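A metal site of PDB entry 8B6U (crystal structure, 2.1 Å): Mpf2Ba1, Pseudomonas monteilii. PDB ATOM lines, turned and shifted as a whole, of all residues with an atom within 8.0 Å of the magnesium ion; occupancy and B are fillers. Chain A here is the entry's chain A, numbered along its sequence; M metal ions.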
ATOM      1  N   ASP A 365      14.158   7.503  28.851  1.00  0.00           N
ATOM      2  CA  ASP A 365      14.881   6.256  29.054  1.00  0.00           C
ATOM      3  C   ASP A 365      15.030   5.559  27.702  1.00  0.00           C
ATOM      4  O   ASP A 365      14.038   5.187  27.090  1.00  0.00           O
ATOM      5  CB  ASP A 365      14.142   5.385  30.074  1.00  0.00           C
ATOM      6  CG  ASP A 365      14.859   4.091  30.454  1.00  0.00           C
ATOM      7  OD1 ASP A 365      15.950   3.857  29.934  1.00  0.00           O
ATOM      8  OD2 ASP A 365      14.284   3.337  31.285  1.00  0.00           O
ATOM      9  N   LEU A 366      16.255   5.480  27.184  1.00  0.00           N
ATOM     10  CA  LEU A 366      16.537   4.850  25.893  1.00  0.00           C
ATOM     11  C   LEU A 366      16.450   3.308  25.971  1.00  0.00           C
ATOM     12  O   LEU A 366      16.855   2.648  25.032  1.00  0.00           O
ATOM     13  CB  LEU A 366      17.958   5.249  25.489  1.00  0.00           C
ATOM     14  CG  LEU A 366      18.156   6.534  24.689  1.00  0.00           C
ATOM     15  CD1 LEU A 366      17.348   7.694  25.206  1.00  0.00           C
ATOM     16  CD2 LEU A 366      19.626   6.880  24.685  1.00  0.00           C
ATOM     17  N   ASN A 367      16.038   2.714  27.117  1.00  0.00           N
ATOM     18  CA  ASN A 367      15.578   1.334  27.185  1.00  0.00           C
ATOM     19  C   ASN A 367      14.127   1.256  27.637  1.00  0.00           C
ATOM     20  O   ASN A 367      13.781   0.321  28.348  1.00  0.00           O
ATOM     21  CB  ASN A 367      16.411   0.467  28.144  1.00  0.00           C
ATOM     22  CG  ASN A 367      17.718   0.080  27.509  1.00  0.00           C
ATOM     23  OD1 ASN A 367      17.860   0.089  26.281  1.00  0.00           O
ATOM     24  ND2 ASN A 367      18.694  -0.231  28.340  1.00  0.00           N
ATOM     25  N   ALA A 368      13.320   2.262  27.242  1.00  0.00           N
ATOM     26  CA  ALA A 368      11.912   2.314  27.596  1.00  0.00           C
ATOM     27  C   ALA A 368      11.189   1.116  26.969  1.00  0.00           C
ATOM     28  O   ALA A 368      11.238   0.914  25.729  1.00  0.00           O
ATOM     29  CB  ALA A 368      11.266   3.639  27.174  1.00  0.00           C
ATOM     30  N   ALA A 370      11.971  -1.989  27.345  1.00  0.00           N
ATOM     31  CA  ALA A 370      12.900  -3.055  26.953  1.00  0.00           C
ATOM     32  C   ALA A 370      13.660  -3.673  28.143  1.00  0.00           C
ATOM     33  O   ALA A 370      14.475  -4.575  27.920  1.00  0.00           O
ATOM     34  CB  ALA A 370      13.893  -2.547  25.917  1.00  0.00           C
ATOM     35  N   GLY A 371      13.437  -3.196  29.386  1.00  0.00           N
ATOM     36  CA  GLY A 371      14.212  -3.643  30.546  1.00  0.00           C
ATOM     37  C   GLY A 371      15.616  -3.027  30.559  1.00  0.00           C
ATOM     38  O   GLY A 371      15.856  -1.999  29.920  1.00  0.00           O
ATOM     39  N   ASP A 373      19.199  -1.214  32.025  1.00  0.00           N
ATOM     40  CA  ASP A 373      19.480   0.059  32.687  1.00  0.00           C
ATOM     41  C   ASP A 373      18.510   1.150  32.247  1.00  0.00           C
ATOM     42  O   ASP A 373      17.928   1.115  31.145  1.00  0.00           O
ATOM     43  CB  ASP A 373      20.896   0.559  32.380  1.00  0.00           C
ATOM     44  CG  ASP A 373      22.013  -0.155  33.133  1.00  0.00           C
ATOM     45  OD1 ASP A 373      21.677  -0.926  34.029  1.00  0.00           O
ATOM     46  OD2 ASP A 373      23.190   0.053  32.781  1.00  0.00           O
ATOM     47  N   ILE A 375      18.751   4.508  30.651  1.00  0.00           N
ATOM     48  CA  ILE A 375      19.788   5.139  29.843  1.00  0.00           C
ATOM     49  C   ILE A 375      19.263   6.503  29.387  1.00  0.00           C
ATOM     50  O   ILE A 375      18.120   6.600  28.937  1.00  0.00           O
ATOM     51  CB  ILE A 375      20.201   4.237  28.672  1.00  0.00           C
ATOM     52  CG1 ILE A 375      20.658   2.857  29.171  1.00  0.00           C
ATOM     53  CG2 ILE A 375      21.239   4.890  27.748  1.00  0.00           C
ATOM     54  CD1 ILE A 375      21.041   1.920  28.040  1.00  0.00           C
ATOM     55  N   ASP A 415      26.485   1.526  24.973  1.00  0.00           N
ATOM     56  CA  ASP A 415      25.479   0.757  24.257  1.00  0.00           C
ATOM     57  C   ASP A 415      24.123   1.259  24.728  1.00  0.00           C
ATOM     58  O   ASP A 415      23.798   1.145  25.927  1.00  0.00           O
ATOM     59  CB  ASP A 415      25.649  -0.767  24.490  1.00  0.00           C
ATOM     60  CG  ASP A 415      24.570  -1.639  23.835  1.00  0.00           C
ATOM     61  OD1 ASP A 415      24.229  -1.346  22.665  1.00  0.00           O
ATOM     62  OD2 ASP A 415      24.051  -2.575  24.513  1.00  0.00           O
ATOM     63  N   LEU A 416      23.327   1.751  23.777  1.00  0.00           N
ATOM     64  CA  LEU A 416      22.007   2.304  24.069  1.00  0.00           C
ATOM     65  C   LEU A 416      20.966   1.193  24.269  1.00  0.00           C
ATOM     66  O   LEU A 416      19.775   1.477  24.429  1.00  0.00           O
ATOM     67  CB  LEU A 416      21.625   3.269  22.934  1.00  0.00           C
ATOM     68  CG  LEU A 416      22.214   4.692  22.972  1.00  0.00           C
ATOM     69  CD1 LEU A 416      23.355   4.858  23.966  1.00  0.00           C
ATOM     70  CD2 LEU A 416      22.608   5.188  21.603  1.00  0.00           C
ATOM     71  N   ASN A 417      21.424  -0.072  24.326  1.00  0.00           N
ATOM     72  CA  ASN A 417      20.584  -1.234  24.624  1.00  0.00           C
ATOM     73  C   ASN A 417      21.058  -2.043  25.838  1.00  0.00           C
ATOM     74  O   ASN A 417      20.578  -3.146  26.069  1.00  0.00           O
ATOM     75  CB  ASN A 417      20.479  -2.139  23.392  1.00  0.00           C
ATOM     76  CG  ASN A 417      19.192  -1.931  22.598  1.00  0.00           C
ATOM     77  OD1 ASN A 417      18.206  -1.423  23.128  1.00  0.00           O
ATOM     78  ND2 ASN A 417      19.179  -2.404  21.359  1.00  0.00           N
ATOM     79  N   LYS A 418      21.932  -1.495  26.671  1.00  0.00           N
ATOM     80  CA  LYS A 418      22.507  -2.292  27.746  1.00  0.00           C
ATOM     81  C   LYS A 418      21.620  -2.312  28.996  1.00  0.00           C
ATOM     82  O   LYS A 418      20.919  -1.356  29.282  1.00  0.00           O
ATOM     83  CB  LYS A 418      23.891  -1.693  28.047  1.00  0.00           C
ATOM     84  CG  LYS A 418      23.890  -0.492  28.972  1.00  0.00           C
ATOM     85  CD  LYS A 418      24.479  -0.788  30.320  1.00  0.00           C
ATOM     86  CE  LYS A 418      25.985  -0.876  30.239  1.00  0.00           C
ATOM     87  NZ  LYS A 418      26.608  -0.712  31.574  1.00  0.00           N
ATOM     88  N   ALA A 420      19.384  -4.647  27.901  1.00  0.00           N
ATOM     89  CA  ALA A 420      18.029  -4.926  27.463  1.00  0.00           C
ATOM     90  C   ALA A 420      18.077  -5.969  26.337  1.00  0.00           C
ATOM     91  O   ALA A 420      17.046  -6.326  25.785  1.00  0.00           O
ATOM     92  CB  ALA A 420      17.379  -3.635  27.010  1.00  0.00           C
ATOM     93  N   GLY A 421      19.301  -6.418  26.021  1.00  0.00           N
ATOM     94  CA  GLY A 421      19.542  -7.349  24.943  1.00  0.00           C
ATOM     95  C   GLY A 421      19.569  -6.643  23.596  1.00  0.00           C
ATOM     96  O   GLY A 421      20.001  -5.494  23.501  1.00  0.00           O
ATOM     97  N   ASP A 423      20.251  -5.720  19.482  1.00  0.00           N
ATOM     98  CA  ASP A 423      21.424  -5.118  18.894  1.00  0.00           C
ATOM     99  C   ASP A 423      22.190  -4.278  19.915  1.00  0.00           C
ATOM    100  O   ASP A 423      21.645  -3.821  20.924  1.00  0.00           O
ATOM    101  CB  ASP A 423      21.064  -4.237  17.705  1.00  0.00           C
ATOM    102  CG  ASP A 423      20.595  -5.055  16.513  1.00  0.00           C
ATOM    103  OD1 ASP A 423      21.209  -6.098  16.274  1.00  0.00           O
ATOM    104  OD2 ASP A 423      19.676  -4.603  15.824  1.00  0.00           O
ATOM    105  N   VAL A 425      23.740  -0.771  20.155  1.00  0.00           N
ATOM    106  CA  VAL A 425      23.393   0.474  19.482  1.00  0.00           C
ATOM    107  C   VAL A 425      24.273   1.611  20.015  1.00  0.00           C
ATOM    108  O   VAL A 425      24.400   1.795  21.224  1.00  0.00           O
ATOM    109  CB  VAL A 425      21.884   0.779  19.620  1.00  0.00           C
ATOM    110  CG1 VAL A 425      21.499   2.105  18.958  1.00  0.00           C
ATOM    111  CG2 VAL A 425      21.058  -0.370  19.071  1.00  0.00           C
ATOM    112  N   ASP A 465      16.443   2.952  15.385  1.00  0.00           N
ATOM    113  CA  ASP A 465      15.712   2.638  16.604  1.00  0.00           C
ATOM    114  C   ASP A 465      16.715   2.361  17.726  1.00  0.00           C
ATOM    115  O   ASP A 465      17.536   1.476  17.575  1.00  0.00           O
ATOM    116  CB  ASP A 465      14.818   1.429  16.311  1.00  0.00           C
ATOM    117  CG  ASP A 465      14.047   0.866  17.483  1.00  0.00           C
ATOM    118  OD1 ASP A 465      13.971   1.544  18.558  1.00  0.00           O
ATOM    119  OD2 ASP A 465      13.503  -0.275  17.313  1.00  0.00           O
ATOM    120  N   LEU A 466      16.591   3.055  18.871  1.00  0.00           N
ATOM    121  CA  LEU A 466      17.532   2.956  19.989  1.00  0.00           C
ATOM    122  C   LEU A 466      17.161   1.801  20.942  1.00  0.00           C
ATOM    123  O   LEU A 466      17.778   1.619  22.025  1.00  0.00           O
ATOM    124  CB  LEU A 466      17.542   4.303  20.736  1.00  0.00           C
ATOM    125  CG  LEU A 466      17.889   5.547  19.901  1.00  0.00           C
ATOM    126  CD1 LEU A 466      18.035   6.775  20.805  1.00  0.00           C
ATOM    127  CD2 LEU A 466      19.140   5.345  19.048  1.00  0.00           C
ATOM    128  N   ASN A 467      16.096   1.073  20.553  1.00  0.00           N
ATOM    129  CA  ASN A 467      15.792  -0.241  21.104  1.00  0.00           C
ATOM    130  C   ASN A 467      15.863  -1.287  19.981  1.00  0.00           C
ATOM    131  O   ASN A 467      15.208  -2.347  20.052  1.00  0.00           O
ATOM    132  CB  ASN A 467      14.430  -0.239  21.816  1.00  0.00           C
ATOM    133  CG  ASN A 467      14.441   0.105  23.287  1.00  0.00           C
ATOM    134  OD1 ASN A 467      15.500   0.211  23.911  1.00  0.00           O
ATOM    135  ND2 ASN A 467      13.235   0.241  23.868  1.00  0.00           N
ATOM    136  N   ARG A 468      16.645  -1.053  18.915  1.00  0.00           N
ATOM    137  CA  ARG A 468      16.638  -2.013  17.804  1.00  0.00           C
ATOM    138  C   ARG A 468      17.094  -3.380  18.321  1.00  0.00           C
ATOM    139  O   ARG A 468      18.059  -3.474  19.115  1.00  0.00           O
ATOM    140  CB  ARG A 468      17.501  -1.592  16.595  1.00  0.00           C
ATOM    141  CG  ARG A 468      16.921  -2.032  15.251  1.00  0.00           C
ATOM    142  CD  ARG A 468      17.802  -1.742  14.044  1.00  0.00           C
ATOM    143  NE  ARG A 468      18.973  -2.608  14.096  1.00  0.00           N
ATOM    144  CZ  ARG A 468      19.993  -2.586  13.254  1.00  0.00           C
ATOM    145  NH1 ARG A 468      20.062  -1.682  12.301  1.00  0.00           N
ATOM    146  NH2 ARG A 468      20.961  -3.478  13.389  1.00  0.00           N
ATOM    147  N   ALA A 470      16.031  -5.237  20.572  1.00  0.00           N
ATOM    148  CA  ALA A 470      15.245  -5.508  21.769  1.00  0.00           C
ATOM    149  C   ALA A 470      13.774  -5.406  21.365  1.00  0.00           C
ATOM    150  O   ALA A 470      13.404  -5.429  20.168  1.00  0.00           O
ATOM    151  CB  ALA A 470      15.609  -4.589  22.900  1.00  0.00           C
ATOM    152  N   GLY A 471      12.928  -5.365  22.372  1.00  0.00           N
ATOM    153  CA  GLY A 471      11.549  -4.982  22.100  1.00  0.00           C
ATOM    154  C   GLY A 471      11.330  -3.558  22.589  1.00  0.00           C
ATOM    155  O   GLY A 471      11.949  -2.596  22.106  1.00  0.00           O
ATOM    156  N   ASN A 473       9.536  -0.004  23.238  1.00  0.00           N
ATOM    157  CA  ASN A 473       9.150   0.987  22.261  1.00  0.00           C
ATOM    158  C   ASN A 473      10.198   1.052  21.157  1.00  0.00           C
ATOM    159  O   ASN A 473      11.370   0.703  21.364  1.00  0.00           O
ATOM    160  CB  ASN A 473       8.899   2.300  22.974  1.00  0.00           C
ATOM    161  CG  ASN A 473       7.926   2.090  24.103  1.00  0.00           C
ATOM    162  OD1 ASN A 473       6.977   1.312  23.965  1.00  0.00           O
ATOM    163  ND2 ASN A 473       8.181   2.833  25.171  1.00  0.00           N
ATOM    164  N   ILE A 475      12.221   3.880  19.441  1.00  0.00           N
ATOM    165  CA  ILE A 475      12.837   5.063  20.047  1.00  0.00           C
ATOM    166  C   ILE A 475      13.763   5.734  19.040  1.00  0.00           C
ATOM    167  O   ILE A 475      14.652   5.082  18.485  1.00  0.00           O
ATOM    168  CB  ILE A 475      13.616   4.694  21.322  1.00  0.00           C
ATOM    169  CG1 ILE A 475      12.740   3.960  22.338  1.00  0.00           C
ATOM    170  CG2 ILE A 475      14.264   5.944  21.936  1.00  0.00           C
ATOM    171  CD1 ILE A 475      13.471   3.597  23.607  1.00  0.00           C
HETATM  172 MG    MG M   1      17.671   0.810  24.097  1.00  0.00          MG
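The magnesium ion is bound by O of Leu 366 (2.2 Å), O of Leu 466 (2.2 Å), O of Leu 416 (2.2 Å), OD1 of Asn 467 (2.3 Å), OD1 of Asn 367 (2.3 Å) and OD1 of Asn 417 (2.5 Å).
The side-chain amide nitrogen (ND2) of Asn 367 sits at hydrogen-bond distance from the backbone carbonyl oxygen (O) of Lys 418, 2.7 Å away. The side-chain amide nitrogen (ND2) of Asn 367 is in hydrogen-bond range of the backbone carbonyl oxygen (O) of Asp 373 (3.2 Å). The backbone carbonyl oxygen (O) of Val 425 sits at hydrogen-bond distance from the backbone NH (N) of Leu 416 (2.8 Å). The side-chain amide nitrogen of Asn 467 is in hydrogen-bond range of the backbone carbonyl oxygen of Asn 473 (3.2 Å). The backbone carbonyl oxygen (O) of Ala 368 is in hydrogen-bond range of the side-chain amide nitrogen (ND2) of Asn 467 (2.8 Å). The backbone carbonyl oxygen (O) of Asp 423 sits at hydrogen-bond distance from the side-chain amide nitrogen (ND2) of Asn 417 (2.9 Å). The backbone carbonyl oxygen (O) of Arg 468 sits at hydrogen-bond distance from the side-chain amide nitrogen (ND2) of Asn 417 (2.7 Å). N of Leu 466 is in hydrogen-bond range of O of Ile 475 (2.8 Å).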
